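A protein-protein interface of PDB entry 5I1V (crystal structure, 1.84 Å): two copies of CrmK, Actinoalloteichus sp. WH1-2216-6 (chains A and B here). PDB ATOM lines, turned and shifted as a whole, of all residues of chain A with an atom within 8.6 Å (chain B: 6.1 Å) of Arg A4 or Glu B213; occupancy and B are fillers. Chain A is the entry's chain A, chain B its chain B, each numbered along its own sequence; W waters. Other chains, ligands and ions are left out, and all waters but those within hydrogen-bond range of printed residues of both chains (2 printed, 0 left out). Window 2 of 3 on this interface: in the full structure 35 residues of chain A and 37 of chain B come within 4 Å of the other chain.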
ATOM      1  N   THR A   3      -4.111 -14.380  13.087  1.00  0.00           N
ATOM      2  CA  THR A   3      -4.892 -13.233  12.555  1.00  0.00           C
ATOM      3  C   THR A   3      -6.298 -13.685  12.164  1.00  0.00           C
ATOM      4  O   THR A   3      -6.495 -14.755  11.562  1.00  0.00           O
ATOM      5  CB  THR A   3      -4.247 -12.554  11.280  1.00  0.00           C
ATOM      6  OG1 THR A   3      -3.141 -13.327  10.782  1.00  0.00           O
ATOM      7  CG2 THR A   3      -3.747 -11.168  11.581  1.00  0.00           C
ATOM      8  N   ARG A   4      -7.265 -12.852  12.505  1.00  0.00           N
ATOM      9  CA  ARG A   4      -8.510 -12.747  11.770  1.00  0.00           C
ATOM     10  C   ARG A   4      -8.244 -12.870  10.240  1.00  0.00           C
ATOM     11  O   ARG A   4      -7.273 -12.313   9.714  1.00  0.00           O
ATOM     12  CB  ARG A   4      -9.094 -11.366  12.076  1.00  0.00           C
ATOM     13  CG  ARG A   4     -10.322 -10.990  11.254  1.00  0.00           C
ATOM     14  CD  ARG A   4     -11.087  -9.831  11.875  1.00  0.00           C
ATOM     15  NE  ARG A   4     -12.518 -10.041  11.635  1.00  0.00           N
ATOM     16  CZ  ARG A   4     -13.267  -9.261  10.873  1.00  0.00           C
ATOM     17  NH1 ARG A   4     -14.548  -9.531  10.681  1.00  0.00           N
ATOM     18  NH2 ARG A   4     -12.736  -8.205  10.314  1.00  0.00           N
ATOM     19  N   ALA A   5      -9.113 -13.585   9.547  1.00  0.00           N
ATOM     20  CA  ALA A   5      -9.006 -13.737   8.117  1.00  0.00           C
ATOM     21  C   ALA A   5      -9.294 -12.398   7.426  1.00  0.00           C
ATOM     22  O   ALA A   5     -10.089 -11.586   7.900  1.00  0.00           O
ATOM     23  CB  ALA A   5      -9.969 -14.804   7.631  1.00  0.00           C
ATOM     24  N   ALA A   6      -8.637 -12.165   6.301  1.00  0.00           N
ATOM     25  CA  ALA A   6      -8.844 -10.951   5.544  1.00  0.00           C
ATOM     26  C   ALA A   6     -10.317 -10.773   5.245  1.00  0.00           C
ATOM     27  O   ALA A   6     -11.019 -11.744   4.989  1.00  0.00           O
ATOM     28  CB  ALA A   6      -8.044 -11.010   4.228  1.00  0.00           C
ATOM     29  N   VAL A   7     -10.789  -9.538   5.242  1.00  0.00           N
ATOM     30  CA  VAL A   7     -12.185  -9.256   4.838  1.00  0.00           C
ATOM     31  C   VAL A   7     -12.345  -9.092   3.343  1.00  0.00           C
ATOM     32  O   VAL A   7     -11.495  -8.504   2.690  1.00  0.00           O
ATOM     33  CB  VAL A   7     -12.699  -8.021   5.598  1.00  0.00           C
ATOM     34  CG1 VAL A   7     -14.114  -7.752   5.181  1.00  0.00           C
ATOM     35  CG2 VAL A   7     -12.650  -8.318   7.096  1.00  0.00           C
ATOM     36  N   THR A   8     -13.424  -9.645   2.775  1.00  0.00           N
ATOM     37  CA  THR A   8     -13.742  -9.459   1.399  1.00  0.00           C
ATOM     38  C   THR A   8     -15.067  -8.721   1.347  1.00  0.00           C
ATOM     39  O   THR A   8     -16.029  -9.132   1.973  1.00  0.00           O
ATOM     40  CB  THR A   8     -13.830 -10.787   0.628  1.00  0.00           C
ATOM     41  OG1 THR A   8     -12.540 -11.404   0.604  1.00  0.00           O
ATOM     42  CG2 THR A   8     -14.279 -10.555  -0.799  1.00  0.00           C
ATOM     43  N   ASP A  13     -22.419  -6.155   0.160  1.00  0.00           N
ATOM     44  CA  ASP A  13     -22.096  -5.734   1.512  1.00  0.00           C
ATOM     45  C   ASP A  13     -22.285  -4.228   1.636  1.00  0.00           C
ATOM     46  O   ASP A  13     -21.907  -3.427   0.751  1.00  0.00           O
ATOM     47  CB  ASP A  13     -20.662  -6.174   1.825  1.00  0.00           C
ATOM     48  CG  ASP A  13     -20.280  -5.955   3.267  1.00  0.00           C
ATOM     49  OD1 ASP A  13     -20.338  -4.805   3.758  1.00  0.00           O
ATOM     50  OD2 ASP A  13     -19.916  -6.936   3.912  1.00  0.00           O
ATOM     51  N   ARG A  15     -20.782  -2.162   3.295  1.00  0.00           N
ATOM     52  CA  ARG A  15     -19.509  -1.448   3.300  1.00  0.00           C
ATOM     53  C   ARG A  15     -18.978  -1.046   1.926  1.00  0.00           C
ATOM     54  O   ARG A  15     -18.111  -0.163   1.822  1.00  0.00           O
ATOM     55  CB  ARG A  15     -18.448  -2.321   3.991  1.00  0.00           C
ATOM     56  CG  ARG A  15     -18.603  -2.388   5.476  1.00  0.00           C
ATOM     57  CD  ARG A  15     -17.633  -3.379   6.047  1.00  0.00           C
ATOM     58  NE  ARG A  15     -18.028  -4.734   5.745  1.00  0.00           N
ATOM     59  CZ  ARG A  15     -17.480  -5.802   6.322  1.00  0.00           C
ATOM     60  NH1 ARG A  15     -16.482  -5.672   7.198  1.00  0.00           N
ATOM     61  NH2 ARG A  15     -17.908  -7.010   5.995  1.00  0.00           N
ATOM     62  N   LEU A  36      -9.549  -6.420   2.530  1.00  0.00           N
ATOM     63  CA  LEU A  36      -8.873  -5.746   3.648  1.00  0.00           C
ATOM     64  C   LEU A  36      -8.032  -6.771   4.434  1.00  0.00           C
ATOM     65  O   LEU A  36      -8.593  -7.503   5.242  1.00  0.00           O
ATOM     66  CB  LEU A  36      -9.902  -5.141   4.589  1.00  0.00           C
ATOM     67  CG  LEU A  36     -10.874  -4.038   4.105  1.00  0.00           C
ATOM     68  CD1 LEU A  36     -10.679  -2.737   4.880  1.00  0.00           C
ATOM     69  CD2 LEU A  36     -10.836  -3.737   2.646  1.00  0.00           C
ATOM     70  N   PRO A  37      -6.721  -6.861   4.140  1.00  0.00           N
ATOM     71  CA  PRO A  37      -5.827  -7.789   4.830  1.00  0.00           C
ATOM     72  C   PRO A  37      -5.341  -7.235   6.172  1.00  0.00           C
ATOM     73  O   PRO A  37      -5.372  -6.023   6.408  1.00  0.00           O
ATOM     74  CB  PRO A  37      -4.699  -7.971   3.836  1.00  0.00           C
ATOM     75  CG  PRO A  37      -4.693  -6.725   3.055  1.00  0.00           C
ATOM     76  CD  PRO A  37      -6.042  -6.142   3.080  1.00  0.00           C
ATOM     77  N   TYR A  38      -4.866  -8.141   7.033  1.00  0.00           N
ATOM     78  CA  TYR A  38      -4.394  -7.770   8.350  1.00  0.00           C
ATOM     79  C   TYR A  38      -2.892  -8.086   8.513  1.00  0.00           C
ATOM     80  O   TYR A  38      -2.326  -7.753   9.537  1.00  0.00           O
ATOM     81  CB  TYR A  38      -5.199  -8.537   9.459  1.00  0.00           C
ATOM     82  CG  TYR A  38      -6.648  -8.136   9.493  1.00  0.00           C
ATOM     83  CD1 TYR A  38      -7.025  -6.906  10.027  1.00  0.00           C
ATOM     84  CD2 TYR A  38      -7.641  -8.947   8.933  1.00  0.00           C
ATOM     85  CE1 TYR A  38      -8.342  -6.502  10.029  1.00  0.00           C
ATOM     86  CE2 TYR A  38      -8.972  -8.556   8.921  1.00  0.00           C
ATOM     87  CZ  TYR A  38      -9.322  -7.321   9.469  1.00  0.00           C
ATOM     88  OH  TYR A  38     -10.626  -6.894   9.463  1.00  0.00           O
ATOM     89  N   SER A  39      -2.251  -8.729   7.534  1.00  0.00           N
ATOM     90  CA  SER A  39      -0.853  -9.123   7.672  1.00  0.00           C
ATOM     91  C   SER A  39      -0.245  -9.177   6.284  1.00  0.00           C
ATOM     92  O   SER A  39      -0.966  -9.277   5.284  1.00  0.00           O
ATOM     93  CB  SER A  39      -0.791 -10.525   8.285  1.00  0.00           C
ATOM     94  OG  SER A  39      -1.386 -11.461   7.385  1.00  0.00           O
ATOM     95  N   GLN A  42      -1.445 -12.113   4.188  1.00  0.00           N
ATOM     96  CA  GLN A  42      -2.741 -11.925   3.566  1.00  0.00           C
ATOM     97  C   GLN A  42      -2.658 -10.981   2.311  1.00  0.00           C
ATOM     98  O   GLN A  42      -3.455 -11.081   1.357  1.00  0.00           O
ATOM     99  CB  GLN A  42      -3.715 -11.443   4.624  1.00  0.00           C
ATOM    100  CG  GLN A  42      -4.137 -12.525   5.575  1.00  0.00           C
ATOM    101  CD  GLN A  42      -5.030 -12.001   6.685  1.00  0.00           C
ATOM    102  OE1 GLN A  42      -5.351 -10.811   6.736  1.00  0.00           O
ATOM    103  NE2 GLN A  42      -5.425 -12.880   7.582  1.00  0.00           N
ATOM    104  N   SER A  83      -6.634  -1.329   7.691  1.00  0.00           N
ATOM    105  CA  SER A  83      -6.548  -2.111   8.918  1.00  0.00           C
ATOM    106  C   SER A  83      -5.113  -2.530   9.305  1.00  0.00           C
ATOM    107  O   SER A  83      -4.945  -3.215  10.280  1.00  0.00           O
ATOM    108  CB  SER A  83      -7.458  -3.356   8.826  1.00  0.00           C
ATOM    109  OG  SER A  83      -8.831  -2.974   8.565  1.00  0.00           O
ATOM    110  N   PHE B  96     -16.753  -6.126  21.886  1.00  0.00           N
ATOM    111  CA  PHE B  96     -15.650  -5.291  21.380  1.00  0.00           C
ATOM    112  C   PHE B  96     -14.951  -4.599  22.536  1.00  0.00           C
ATOM    113  O   PHE B  96     -15.587  -3.861  23.287  1.00  0.00           O
ATOM    114  CB  PHE B  96     -16.188  -4.233  20.413  1.00  0.00           C
ATOM    115  CG  PHE B  96     -16.698  -4.841  19.147  1.00  0.00           C
ATOM    116  CD1 PHE B  96     -15.828  -5.088  18.081  1.00  0.00           C
ATOM    117  CD2 PHE B  96     -17.995  -5.195  19.033  1.00  0.00           C
ATOM    118  CE1 PHE B  96     -16.299  -5.670  16.922  1.00  0.00           C
ATOM    119  CE2 PHE B  96     -18.488  -5.760  17.873  1.00  0.00           C
ATOM    120  CZ  PHE B  96     -17.637  -6.017  16.816  1.00  0.00           C
ATOM    121  N   LYS B 113     -15.353  -0.516   9.305  1.00  0.00           N
ATOM    122  CA  LYS B 113     -14.698  -1.124   8.139  1.00  0.00           C
ATOM    123  C   LYS B 113     -14.417  -2.622   8.373  1.00  0.00           C
ATOM    124  O   LYS B 113     -14.608  -3.451   7.471  1.00  0.00           O
ATOM    125  CB  LYS B 113     -13.438  -0.369   7.746  1.00  0.00           C
ATOM    126  CG  LYS B 113     -13.696   1.100   7.442  1.00  0.00           C
ATOM    127  CD  LYS B 113     -12.408   1.839   7.151  1.00  0.00           C
ATOM    128  CE  LYS B 113     -12.679   3.086   6.323  1.00  0.00           C
ATOM    129  NZ  LYS B 113     -11.403   3.434   5.660  1.00  0.00           N
ATOM    130  N   ASN B 114     -14.017  -2.990   9.580  1.00  0.00           N
ATOM    131  CA  ASN B 114     -13.649  -4.385   9.832  1.00  0.00           C
ATOM    132  C   ASN B 114     -14.823  -5.334  10.054  1.00  0.00           C
ATOM    133  O   ASN B 114     -14.745  -6.518   9.723  1.00  0.00           O
ATOM    134  CB  ASN B 114     -12.694  -4.484  11.018  1.00  0.00           C
ATOM    135  CG  ASN B 114     -11.355  -3.869  10.689  1.00  0.00           C
ATOM    136  OD1 ASN B 114     -10.620  -4.437   9.906  1.00  0.00           O
ATOM    137  ND2 ASN B 114     -11.101  -2.661  11.157  1.00  0.00           N
ATOM    138  N   TYR B 115     -15.897  -4.822  10.606  1.00  0.00           N
ATOM    139  CA  TYR B 115     -17.031  -5.679  10.971  1.00  0.00           C
ATOM    140  C   TYR B 115     -18.398  -5.226  10.478  1.00  0.00           C
ATOM    141  O   TYR B 115     -19.352  -5.961  10.605  1.00  0.00           O
ATOM    142  CB  TYR B 115     -17.087  -5.724  12.477  1.00  0.00           C
ATOM    143  CG  TYR B 115     -15.827  -6.084  13.139  1.00  0.00           C
ATOM    144  CD1 TYR B 115     -15.450  -7.399  13.242  1.00  0.00           C
ATOM    145  CD2 TYR B 115     -14.999  -5.121  13.673  1.00  0.00           C
ATOM    146  CE1 TYR B 115     -14.277  -7.748  13.851  1.00  0.00           C
ATOM    147  CE2 TYR B 115     -13.847  -5.476  14.312  1.00  0.00           C
ATOM    148  CZ  TYR B 115     -13.500  -6.789  14.391  1.00  0.00           C
ATOM    149  OH  TYR B 115     -12.330  -7.148  15.018  1.00  0.00           O
ATOM    150  N   GLY B 116     -18.509  -3.990  10.027  1.00  0.00           N
ATOM    151  CA  GLY B 116     -19.776  -3.443   9.545  1.00  0.00           C
ATOM    152  C   GLY B 116     -20.701  -2.956  10.676  1.00  0.00           C
ATOM    153  O   GLY B 116     -21.882  -2.743  10.463  1.00  0.00           O
ATOM    154  N   VAL B 117     -20.167  -2.740  11.874  1.00  0.00           N
ATOM    155  CA  VAL B 117     -21.025  -2.476  13.052  1.00  0.00           C
ATOM    156  C   VAL B 117     -20.700  -1.071  13.587  1.00  0.00           C
ATOM    157  O   VAL B 117     -19.702  -0.453  13.180  1.00  0.00           O
ATOM    158  CB  VAL B 117     -20.913  -3.547  14.135  1.00  0.00           C
ATOM    159  CG1 VAL B 117     -21.182  -4.961  13.645  1.00  0.00           C
ATOM    160  CG2 VAL B 117     -19.594  -3.481  14.842  1.00  0.00           C
ATOM    161  N   ALA B 211     -20.605 -14.060  16.412  1.00  0.00           N
ATOM    162  CA  ALA B 211     -19.824 -13.382  15.375  1.00  0.00           C
ATOM    163  C   ALA B 211     -19.812 -11.903  15.700  1.00  0.00           C
ATOM    164  O   ALA B 211     -20.821 -11.352  16.139  1.00  0.00           O
ATOM    165  CB  ALA B 211     -20.415 -13.621  13.997  1.00  0.00           C
ATOM    166  N   PRO B 212     -18.658 -11.253  15.502  1.00  0.00           N
ATOM    167  CA  PRO B 212     -18.563  -9.837  15.733  1.00  0.00           C
ATOM    168  C   PRO B 212     -19.523  -9.035  14.906  1.00  0.00           C
ATOM    169  O   PRO B 212     -19.970  -7.963  15.314  1.00  0.00           O
ATOM    170  CB  PRO B 212     -17.103  -9.507  15.329  1.00  0.00           C
ATOM    171  CG  PRO B 212     -16.536 -10.753  14.694  1.00  0.00           C
ATOM    172  CD  PRO B 212     -17.347 -11.875  15.250  1.00  0.00           C
ATOM    173  N   GLU B 213     -19.871  -9.529  13.728  1.00  0.00           N
ATOM    174  CA  GLU B 213     -20.699  -8.756  12.841  1.00  0.00           C
ATOM    175  C   GLU B 213     -22.106  -8.629  13.404  1.00  0.00           C
ATOM    176  O   GLU B 213     -22.881  -7.825  12.941  1.00  0.00           O
ATOM    177  CB  GLU B 213     -20.732  -9.381  11.453  1.00  0.00           C
ATOM    178  CG  GLU B 213     -19.395  -9.273  10.713  1.00  0.00           C
ATOM    179  CD  GLU B 213     -18.341 -10.313  11.108  1.00  0.00           C
ATOM    180  OE1 GLU B 213     -18.627 -11.286  11.863  1.00  0.00           O
ATOM    181  OE2 GLU B 213     -17.185 -10.145  10.639  1.00  0.00           O
ATOM    182  N   GLU B 214     -22.425  -9.488  14.355  1.00  0.00           N
ATOM    183  CA  GLU B 214     -23.724  -9.481  15.067  1.00  0.00           C
ATOM    184  C   GLU B 214     -23.676  -8.924  16.508  1.00  0.00           C
ATOM    185  O   GLU B 214     -24.705  -8.828  17.163  1.00  0.00           O
ATOM    186  CB  GLU B 214     -24.230 -10.933  15.188  1.00  0.00           C
ATOM    187  CG  GLU B 214     -24.297 -11.706  13.889  1.00  0.00           C
ATOM    188  CD  GLU B 214     -25.283 -11.123  12.924  1.00  0.00           C
ATOM    189  OE1 GLU B 214     -26.469 -11.002  13.309  1.00  0.00           O
ATOM    190  OE2 GLU B 214     -24.891 -10.816  11.777  1.00  0.00           O
ATOM    191  N   ALA B 215     -22.483  -8.602  17.007  1.00  0.00           N
ATOM    192  CA  ALA B 215     -22.309  -8.232  18.408  1.00  0.00           C
ATOM    193  C   ALA B 215     -22.680  -6.778  18.690  1.00  0.00           C
ATOM    194  O   ALA B 215     -22.927  -6.412  19.837  1.00  0.00           O
ATOM    195  CB  ALA B 215     -20.898  -8.570  18.842  1.00  0.00           C
ATOM    196  N   LEU B 216     -22.738  -5.936  17.654  1.00  0.00           N
ATOM    197  CA  LEU B 216     -23.179  -4.569  17.775  1.00  0.00           C
ATOM    198  C   LEU B 216     -24.096  -4.309  16.581  1.00  0.00           C
ATOM    199  O   LEU B 216     -24.070  -5.071  15.592  1.00  0.00           O
ATOM    200  CB  LEU B 216     -21.992  -3.612  17.818  1.00  0.00           C
ATOM    201  CG  LEU B 216     -21.229  -3.316  19.117  1.00  0.00           C
ATOM    202  CD1 LEU B 216     -20.158  -2.258  18.866  1.00  0.00           C
ATOM    203  CD2 LEU B 216     -22.126  -2.874  20.259  1.00  0.00           C
ATOM    204  N   PRO B 217     -24.889  -3.237  16.631  1.00  0.00           N
ATOM    205  CA  PRO B 217     -25.842  -3.046  15.539  1.00  0.00           C
ATOM    206  C   PRO B 217     -25.179  -2.612  14.247  1.00  0.00           C
ATOM    207  O   PRO B 217     -24.150  -1.933  14.290  1.00  0.00           O
ATOM    208  CB  PRO B 217     -26.748  -1.929  16.036  1.00  0.00           C
ATOM    209  CG  PRO B 217     -26.492  -1.810  17.496  1.00  0.00           C
ATOM    210  CD  PRO B 217     -25.138  -2.338  17.767  1.00  0.00           C
ATOM    211  N   ARG B 218     -25.760  -2.980  13.107  1.00  0.00           N
ATOM    212  CA  ARG B 218     -25.323  -2.391  11.809  1.00  0.00           C
ATOM    213  C   ARG B 218     -26.015  -1.083  11.572  1.00  0.00           C
ATOM    214  O   ARG B 218     -27.214  -1.047  11.686  1.00  0.00           O
ATOM    215  CB  ARG B 218     -25.715  -3.310  10.672  1.00  0.00           C
ATOM    216  CG  ARG B 218     -25.050  -4.649  10.839  1.00  0.00           C
ATOM    217  CD  ARG B 218     -25.137  -5.508   9.585  1.00  0.00           C
ATOM    218  NE  ARG B 218     -24.706  -6.841   9.992  1.00  0.00           N
ATOM    219  CZ  ARG B 218     -24.884  -7.963   9.314  1.00  0.00           C
ATOM    220  NH1 ARG B 218     -25.484  -7.960   8.124  1.00  0.00           N
ATOM    221  NH2 ARG B 218     -24.450  -9.103   9.847  1.00  0.00           N
HETATM  222  O   HOH W   1     -16.613  -8.824   7.985  1.00  0.00           O
HETATM  223  O   HOH W   2     -15.859 -12.348  11.765  1.00  0.00           O
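O of Asn B114 is in hydrogen-bond range of NH2 of Arg A4 (2.7 Å).
The guanidinium group of Arg A4 is in salt-bridge range of the side-chain carboxylate of Glu B213.
The guanidinium group (NH1) of Arg A15 lies within hydrogen-bond range of the backbone carbonyl oxygen (O) of Lys B113, 2.9 Å away.
The guanidinium group of Arg A15 is in hydrogen-bond range of the backbone carbonyl oxygen of Asn B114 (3.2 Å).
OH of Tyr A38 sits at hydrogen-bond distance from OD1 of Asn B114 (2.5 Å).
The side-chain amide oxygen (OD1) of Asn B114 lies within hydrogen-bond range of the side-chain hydroxyl (OG) of Ser A83 (2.7 Å).
The guanidinium group (NH2) of Arg A4 is in hydrogen-bond range of the side-chain hydroxyl (OH) of Tyr A38 (2.6 Å).
NE2 of Gln A42 lies within hydrogen-bond range of O of Arg A4 (2.9 Å).
The backbone carbonyl oxygen (O) of Val A7 lies within hydrogen-bond range of the backbone NH (N) of Leu A36 (2.9 Å).
NH2 of Arg A15 is in salt-bridge range of OD2 of Asp A13 (2.9 Å).
N of Tyr A38 sits at hydrogen-bond distance from OE1 of Gln A42, at 2.7 Å.
Among the printed residues, merely in contact across the chains: Arg A4 with Tyr B115 (3.5 Å), Val A7 with Asn B114 (3.8 Å), Arg A15 with Tyr B115 (3.6 Å) and Arg A15 with Gly B116 (3.9 Å).
Arg A4 touches three residues of chain B.
Of the printed residues of chain A, Lys B113 touches Arg A15 (2.9 Å).
Of the printed residues of chain A, Gly B116 touches Arg A15 (3.9 Å).
Val B117 touches none of the printed residues of chain A.
Of chain A, only Arg A4 comes within 4 Å of Glu B213.
The nearest residue of chain B that does not touch Arg A4 is Pro B212 (4.6 Å).
The nearest printed residue of chain B that does not touch Tyr A38 is Lys B113 (5.6 Å).
Of the 14 printed residues of chain B, 5 touch a printed residue of chain A.
Printed residues of chain B that touch a printed residue of chain A: Lys B113, Asn B114, Tyr B115, Gly B116 and Glu B213.
Of the 14 printed residues of chain A, 5 touch a printed residue of chain B.
Printed residues of chain A that touch a printed residue of chain B: Arg A4, Val A7, Arg A15, Tyr A38 and Ser A83.
No position is printed for both chains.
Of the 10 pairs that touch across the chains among the printed residues, none has its exchanged pair printed and touching as well.
Water W2 lies within hydrogen-bond range of the side-chain carboxylate (OE2) of Glu B213 (2.8 Å) and the guanidinium group (NH1) of Arg A4 (3.3 Å).
Water W1 lies within hydrogen-bond range of NH2 of Arg A15 (3.0 Å), OE2 of Glu B213 (3.0 Å), O of Asn B114 (3.4 Å) and NH1 of Arg A4 (3.5 Å).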
